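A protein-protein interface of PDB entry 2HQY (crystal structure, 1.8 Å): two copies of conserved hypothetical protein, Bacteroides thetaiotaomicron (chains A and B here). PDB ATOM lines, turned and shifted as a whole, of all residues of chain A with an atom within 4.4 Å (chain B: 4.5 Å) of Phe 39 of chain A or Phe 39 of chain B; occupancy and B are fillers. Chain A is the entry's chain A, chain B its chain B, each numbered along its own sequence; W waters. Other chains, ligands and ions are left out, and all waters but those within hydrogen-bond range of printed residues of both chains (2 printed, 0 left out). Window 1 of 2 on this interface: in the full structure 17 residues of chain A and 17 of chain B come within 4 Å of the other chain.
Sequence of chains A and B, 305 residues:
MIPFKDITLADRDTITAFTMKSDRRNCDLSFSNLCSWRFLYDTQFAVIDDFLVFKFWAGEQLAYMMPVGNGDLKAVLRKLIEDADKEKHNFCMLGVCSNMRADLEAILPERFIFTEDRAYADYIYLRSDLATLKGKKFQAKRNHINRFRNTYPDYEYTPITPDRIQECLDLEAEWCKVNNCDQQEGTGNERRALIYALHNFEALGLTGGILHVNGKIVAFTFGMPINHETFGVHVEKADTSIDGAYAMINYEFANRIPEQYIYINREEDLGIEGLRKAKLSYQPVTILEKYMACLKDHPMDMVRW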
ATOM      1  N   SER A  36     -14.730  26.610  -1.099  1.00  0.00           N
ATOM      2  CA  SER A  36     -14.266  26.120  -2.408  1.00  0.00           C
ATOM      3  C   SER A  36     -12.747  26.188  -2.530  1.00  0.00           C
ATOM      4  O   SER A  36     -12.153  25.407  -3.273  1.00  0.00           O
ATOM      5  CB  SER A  36     -14.907  26.891  -3.584  1.00  0.00           C
ATOM      6  OG  SER A  36     -16.321  26.731  -3.636  1.00  0.00           O
ATOM      7  N   TRP A  37     -12.127  27.130  -1.807  1.00  0.00           N
ATOM      8  CA  TRP A  37     -10.657  27.258  -1.802  1.00  0.00           C
ATOM      9  C   TRP A  37      -9.957  26.580  -0.619  1.00  0.00           C
ATOM     10  O   TRP A  37      -8.721  26.660  -0.477  1.00  0.00           O
ATOM     11  CB  TRP A  37     -10.226  28.740  -1.950  1.00  0.00           C
ATOM     12  CG  TRP A  37     -10.469  29.244  -3.376  1.00  0.00           C
ATOM     13  CD1 TRP A  37     -11.620  29.786  -3.872  1.00  0.00           C
ATOM     14  CD2 TRP A  37      -9.550  29.174  -4.473  1.00  0.00           C
ATOM     15  NE1 TRP A  37     -11.465  30.087  -5.217  1.00  0.00           N
ATOM     16  CE2 TRP A  37     -10.204  29.722  -5.609  1.00  0.00           C
ATOM     17  CE3 TRP A  37      -8.226  28.736  -4.600  1.00  0.00           C
ATOM     18  CZ2 TRP A  37      -9.580  29.821  -6.862  1.00  0.00           C
ATOM     19  CZ3 TRP A  37      -7.596  28.846  -5.850  1.00  0.00           C
ATOM     20  CH2 TRP A  37      -8.286  29.386  -6.966  1.00  0.00           C
ATOM     21  N   ARG A  38     -10.740  25.906   0.234  1.00  0.00           N
ATOM     22  CA  ARG A  38     -10.168  25.210   1.393  1.00  0.00           C
ATOM     23  C   ARG A  38      -9.097  24.172   0.971  1.00  0.00           C
ATOM     24  O   ARG A  38      -8.139  23.907   1.704  1.00  0.00           O
ATOM     25  CB  ARG A  38     -11.289  24.528   2.179  1.00  0.00           C
ATOM     26  CG  ARG A  38     -10.845  23.864   3.520  1.00  0.00           C
ATOM     27  CD  ARG A  38     -11.969  22.966   4.058  1.00  0.00           C
ATOM     28  NE  ARG A  38     -12.257  21.919   3.080  1.00  0.00           N
ATOM     29  CZ  ARG A  38     -13.425  21.318   2.914  1.00  0.00           C
ATOM     30  NH1 ARG A  38     -14.459  21.612   3.705  1.00  0.00           N
ATOM     31  NH2 ARG A  38     -13.532  20.383   1.956  1.00  0.00           N
ATOM     32  N   PHE A  39      -9.282  23.579  -0.209  1.00  0.00           N
ATOM     33  CA  PHE A  39      -8.371  22.534  -0.701  1.00  0.00           C
ATOM     34  C   PHE A  39      -6.955  23.131  -0.828  1.00  0.00           C
ATOM     35  O   PHE A  39      -5.987  22.411  -0.752  1.00  0.00           O
ATOM     36  CB  PHE A  39      -8.816  22.003  -2.068  1.00  0.00           C
ATOM     37  CG  PHE A  39      -8.410  22.894  -3.198  1.00  0.00           C
ATOM     38  CD1 PHE A  39      -7.182  22.706  -3.858  1.00  0.00           C
ATOM     39  CD2 PHE A  39      -9.208  23.999  -3.553  1.00  0.00           C
ATOM     40  CE1 PHE A  39      -6.764  23.608  -4.900  1.00  0.00           C
ATOM     41  CE2 PHE A  39      -8.786  24.922  -4.565  1.00  0.00           C
ATOM     42  CZ  PHE A  39      -7.562  24.712  -5.243  1.00  0.00           C
ATOM     43  N   LEU A  40      -6.857  24.447  -1.038  1.00  0.00           N
ATOM     44  CA  LEU A  40      -5.538  25.048  -1.268  1.00  0.00           C
ATOM     45  C   LEU A  40      -4.912  25.546   0.049  1.00  0.00           C
ATOM     46  O   LEU A  40      -3.670  25.553   0.214  1.00  0.00           O
ATOM     47  CB  LEU A  40      -5.658  26.196  -2.270  1.00  0.00           C
ATOM     48  CG  LEU A  40      -4.336  26.823  -2.771  1.00  0.00           C
ATOM     49  CD1 LEU A  40      -3.429  25.730  -3.381  1.00  0.00           C
ATOM     50  CD2 LEU A  40      -4.638  27.908  -3.809  1.00  0.00           C
ATOM     51  N   TYR A  41      -5.760  26.022   0.956  1.00  0.00           N
ATOM     52  CA  TYR A  41      -5.278  26.743   2.166  1.00  0.00           C
ATOM     53  C   TYR A  41      -5.493  26.039   3.499  1.00  0.00           C
ATOM     54  O   TYR A  41      -5.171  26.595   4.551  1.00  0.00           O
ATOM     55  CB  TYR A  41      -5.961  28.111   2.233  1.00  0.00           C
ATOM     56  CG  TYR A  41      -5.706  28.940   0.998  1.00  0.00           C
ATOM     57  CD1 TYR A  41      -4.396  29.272   0.621  1.00  0.00           C
ATOM     58  CD2 TYR A  41      -6.765  29.399   0.212  1.00  0.00           C
ATOM     59  CE1 TYR A  41      -4.158  30.047  -0.536  1.00  0.00           C
ATOM     60  CE2 TYR A  41      -6.536  30.170  -0.944  1.00  0.00           C
ATOM     61  CZ  TYR A  41      -5.232  30.481  -1.304  1.00  0.00           C
ATOM     62  OH  TYR A  41      -4.990  31.243  -2.439  1.00  0.00           O
ATOM     63  N   ASN A 189      -5.755  25.291 -10.052  1.00  0.00           N
ATOM     64  CA  ASN A 189      -6.331  25.566  -8.742  1.00  0.00           C
ATOM     65  C   ASN A 189      -7.757  26.101  -8.881  1.00  0.00           C
ATOM     66  O   ASN A 189      -8.651  25.712  -8.130  1.00  0.00           O
ATOM     67  CB  ASN A 189      -5.441  26.565  -7.978  1.00  0.00           C
ATOM     68  CG  ASN A 189      -4.179  25.899  -7.422  1.00  0.00           C
ATOM     69  OD1 ASN A 189      -4.131  24.684  -7.288  1.00  0.00           O
ATOM     70  ND2 ASN A 189      -3.183  26.699  -7.060  1.00  0.00           N
ATOM     71  N   ARG A 192     -10.193  23.265  -9.339  1.00  0.00           N
ATOM     72  CA  ARG A 192     -10.552  22.563  -8.073  1.00  0.00           C
ATOM     73  C   ARG A 192     -11.657  23.311  -7.308  1.00  0.00           C
ATOM     74  O   ARG A 192     -12.612  22.696  -6.799  1.00  0.00           O
ATOM     75  CB  ARG A 192      -9.311  22.393  -7.184  1.00  0.00           C
ATOM     76  CG  ARG A 192      -8.284  21.387  -7.749  1.00  0.00           C
ATOM     77  CD  ARG A 192      -8.865  19.938  -7.831  1.00  0.00           C
ATOM     78  NE  ARG A 192      -9.586  19.581  -6.608  1.00  0.00           N
ATOM     79  CZ  ARG A 192      -9.039  19.249  -5.436  1.00  0.00           C
ATOM     80  NH1 ARG A 192      -7.699  19.165  -5.277  1.00  0.00           N
ATOM     81  NH2 ARG A 192      -9.856  18.973  -4.414  1.00  0.00           N
ATOM     82  N   ALA A 193     -11.529  24.633  -7.228  1.00  0.00           N
ATOM     83  CA  ALA A 193     -12.526  25.445  -6.512  1.00  0.00           C
ATOM     84  C   ALA A 193     -13.864  25.469  -7.251  1.00  0.00           C
ATOM     85  O   ALA A 193     -14.927  25.337  -6.635  1.00  0.00           O
ATOM     86  CB  ALA A 193     -12.001  26.852  -6.298  1.00  0.00           C
ATOM     87  N   SER B  36      -6.377  14.115   6.014  1.00  0.00           N
ATOM     88  CA  SER B  36      -5.169  14.709   5.442  1.00  0.00           C
ATOM     89  C   SER B  36      -5.251  14.701   3.917  1.00  0.00           C
ATOM     90  O   SER B  36      -4.554  15.489   3.254  1.00  0.00           O
ATOM     91  CB  SER B  36      -3.909  13.962   5.905  1.00  0.00           C
ATOM     92  OG  SER B  36      -3.723  14.170   7.302  1.00  0.00           O
ATOM     93  N   TRP B  37      -6.083  13.787   3.362  1.00  0.00           N
ATOM     94  CA  TRP B  37      -6.229  13.722   1.895  1.00  0.00           C
ATOM     95  C   TRP B  37      -7.481  14.404   1.355  1.00  0.00           C
ATOM     96  O   TRP B  37      -7.740  14.432   0.148  1.00  0.00           O
ATOM     97  CB  TRP B  37      -6.069  12.266   1.389  1.00  0.00           C
ATOM     98  CG  TRP B  37      -4.632  11.815   1.501  1.00  0.00           C
ATOM     99  CD1 TRP B  37      -4.034  11.223   2.576  1.00  0.00           C
ATOM    100  CD2 TRP B  37      -3.625  11.944   0.500  1.00  0.00           C
ATOM    101  NE1 TRP B  37      -2.705  10.944   2.296  1.00  0.00           N
ATOM    102  CE2 TRP B  37      -2.431  11.378   1.024  1.00  0.00           C
ATOM    103  CE3 TRP B  37      -3.617  12.451  -0.816  1.00  0.00           C
ATOM    104  CZ2 TRP B  37      -1.225  11.340   0.290  1.00  0.00           C
ATOM    105  CZ3 TRP B  37      -2.426  12.393  -1.552  1.00  0.00           C
ATOM    106  CH2 TRP B  37      -1.250  11.847  -0.999  1.00  0.00           C
ATOM    107  N   ARG B  38      -8.228  15.024   2.263  1.00  0.00           N
ATOM    108  CA  ARG B  38      -9.418  15.747   1.844  1.00  0.00           C
ATOM    109  C   ARG B  38      -9.109  16.824   0.784  1.00  0.00           C
ATOM    110  O   ARG B  38      -9.914  17.025  -0.111  1.00  0.00           O
ATOM    111  CB  ARG B  38     -10.094  16.387   3.067  1.00  0.00           C
ATOM    112  CG  ARG B  38     -11.444  17.070   2.750  1.00  0.00           C
ATOM    113  CD  ARG B  38     -11.942  17.890   4.004  1.00  0.00           C
ATOM    114  NE  ARG B  38     -10.964  18.986   4.169  1.00  0.00           N
ATOM    115  CZ  ARG B  38     -10.722  19.644   5.292  1.00  0.00           C
ATOM    116  NH1 ARG B  38     -11.406  19.352   6.406  1.00  0.00           N
ATOM    117  NH2 ARG B  38      -9.799  20.630   5.269  1.00  0.00           N
ATOM    118  N   PHE B  39      -7.950  17.511   0.894  1.00  0.00           N
ATOM    119  CA  PHE B  39      -7.572  18.569  -0.079  1.00  0.00           C
ATOM    120  C   PHE B  39      -7.588  18.021  -1.522  1.00  0.00           C
ATOM    121  O   PHE B  39      -7.707  18.799  -2.451  1.00  0.00           O
ATOM    122  CB  PHE B  39      -6.145  19.130   0.191  1.00  0.00           C
ATOM    123  CG  PHE B  39      -5.046  18.206  -0.293  1.00  0.00           C
ATOM    124  CD1 PHE B  39      -4.471  18.392  -1.561  1.00  0.00           C
ATOM    125  CD2 PHE B  39      -4.630  17.121   0.482  1.00  0.00           C
ATOM    126  CE1 PHE B  39      -3.494  17.528  -2.049  1.00  0.00           C
ATOM    127  CE2 PHE B  39      -3.632  16.238  -0.002  1.00  0.00           C
ATOM    128  CZ  PHE B  39      -3.078  16.432  -1.282  1.00  0.00           C
ATOM    129  N   LEU B  40      -7.351  16.720  -1.700  1.00  0.00           N
ATOM    130  CA  LEU B  40      -7.249  16.107  -3.042  1.00  0.00           C
ATOM    131  C   LEU B  40      -8.603  15.585  -3.540  1.00  0.00           C
ATOM    132  O   LEU B  40      -8.890  15.619  -4.771  1.00  0.00           O
ATOM    133  CB  LEU B  40      -6.218  14.944  -3.055  1.00  0.00           C
ATOM    134  CG  LEU B  40      -5.834  14.444  -4.463  1.00  0.00           C
ATOM    135  CD1 LEU B  40      -5.246  15.575  -5.322  1.00  0.00           C
ATOM    136  CD2 LEU B  40      -4.849  13.255  -4.351  1.00  0.00           C
ATOM    137  N   TYR B  41      -9.440  15.108  -2.611  1.00  0.00           N
ATOM    138  CA  TYR B  41     -10.653  14.367  -3.007  1.00  0.00           C
ATOM    139  C   TYR B  41     -11.992  15.039  -2.644  1.00  0.00           C
ATOM    140  O   TYR B  41     -13.068  14.477  -2.930  1.00  0.00           O
ATOM    141  CB  TYR B  41     -10.617  12.974  -2.366  1.00  0.00           C
ATOM    142  CG  TYR B  41      -9.403  12.183  -2.741  1.00  0.00           C
ATOM    143  CD1 TYR B  41      -9.098  11.931  -4.088  1.00  0.00           C
ATOM    144  CD2 TYR B  41      -8.590  11.626  -1.761  1.00  0.00           C
ATOM    145  CE1 TYR B  41      -7.993  11.158  -4.448  1.00  0.00           C
ATOM    146  CE2 TYR B  41      -7.468  10.868  -2.101  1.00  0.00           C
ATOM    147  CZ  TYR B  41      -7.189  10.632  -3.444  1.00  0.00           C
ATOM    148  OH  TYR B  41      -6.089   9.902  -3.787  1.00  0.00           O
ATOM    149  N   ASN B 189       1.427  16.179  -3.769  1.00  0.00           N
ATOM    150  CA  ASN B 189       0.225  15.760  -3.050  1.00  0.00           C
ATOM    151  C   ASN B 189       0.559  15.116  -1.714  1.00  0.00           C
ATOM    152  O   ASN B 189      -0.042  15.446  -0.680  1.00  0.00           O
ATOM    153  CB  ASN B 189      -0.596  14.820  -3.912  1.00  0.00           C
ATOM    154  CG  ASN B 189      -1.318  15.546  -5.039  1.00  0.00           C
ATOM    155  OD1 ASN B 189      -1.452  16.769  -5.024  1.00  0.00           O
ATOM    156  ND2 ASN B 189      -1.791  14.792  -6.005  1.00  0.00           N
ATOM    157  N   ARG B 192       1.357  17.861   0.744  1.00  0.00           N
ATOM    158  CA  ARG B 192       0.161  18.542   1.272  1.00  0.00           C
ATOM    159  C   ARG B 192      -0.468  17.743   2.404  1.00  0.00           C
ATOM    160  O   ARG B 192      -0.922  18.309   3.414  1.00  0.00           O
ATOM    161  CB  ARG B 192      -0.903  18.743   0.165  1.00  0.00           C
ATOM    162  CG  ARG B 192      -0.503  19.757  -0.887  1.00  0.00           C
ATOM    163  CD  ARG B 192      -0.469  21.197  -0.328  1.00  0.00           C
ATOM    164  NE  ARG B 192      -1.630  21.470   0.520  1.00  0.00           N
ATOM    165  CZ  ARG B 192      -2.845  21.804   0.074  1.00  0.00           C
ATOM    166  NH1 ARG B 192      -3.103  21.906  -1.269  1.00  0.00           N
ATOM    167  NH2 ARG B 192      -3.827  22.008   0.983  1.00  0.00           N
ATOM    168  N   ALA B 193      -0.533  16.424   2.208  1.00  0.00           N
ATOM    169  CA  ALA B 193      -1.108  15.527   3.206  1.00  0.00           C
ATOM    170  C   ALA B 193      -0.223  15.438   4.460  1.00  0.00           C
ATOM    171  O   ALA B 193      -0.732  15.450   5.581  1.00  0.00           O
ATOM    172  CB  ALA B 193      -1.335  14.156   2.599  1.00  0.00           C
HETATM  173  O   HOH W   1     -10.039  20.570   1.817  1.00  0.00           O
HETATM  174  O   HOH W   2     -11.520  16.317  -5.782  1.00  0.00           O
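O of Phe 39 of chain A is in hydrogen-bond range of NH2 of Arg 192 of chain B (2.8 Å). The guanidinium group (NH1) of Arg 192 of chain A sits at hydrogen-bond distance from the backbone carbonyl oxygen (O) of Phe 39 of chain B (2.8 Å). NE of Arg 38 of chain A lies close to NE of Arg 38 of chain B.
Phe 39 of chain B touches two residues of chain A. Printed residues of chain B within 4 Å of Arg 192 of chain A: Phe 39 and Leu 40. Of the printed residues of chain B, Arg 38 of chain A touches Arg 38 (3.4 Å). Of the printed residues of chain A, Arg 192 of chain B touches Phe 39 and Leu 40. Printed residues of chain A within 4 Å of Leu 40 of chain B: Arg 192 (3.5 Å). Ala 193 of chain A touches none of the printed residues of chain B.
Among the printed residues, merely in contact across the chains: Phe 39 of chain A with Phe 39 of chain B, Leu 40 of chain A with Arg 192 of chain B and Arg 192 of chain A with Leu 40 of chain B.
Of the 9 printed residues of chain A, 4 touch a printed residue of chain B. Among the printed residues, no Asp or Glu carboxylate lies within 4 Å of a Lys or Arg side-chain nitrogen of the other chain.
Water W1 lies within hydrogen-bond range of NE of Arg 38 of chain A and NE of Arg 38 of chain B. Water W2 lies within hydrogen-bond range of O of Leu 40 of chain B (2.9 Å) and NH2 of Arg 192 of chain A (3.4 Å).
Arg 38 of chain A touches its own counterpart, Arg 38 of chain B. Phe 39 of chain A touches its own counterpart, Phe 39 of chain B. Phe 39 of chain A touches Arg 192 of chain B, and with the chains exchanged Arg 192 of chain A touches Phe 39 of chain B. Leu 40 of chain A touches Arg 192 of chain B, and with the chains exchanged Arg 192 of chain A touches Leu 40 of chain B. Of the 6 pairs that touch across the chains among the printed residues, 6 have their exchanged pair printed and touching as well.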
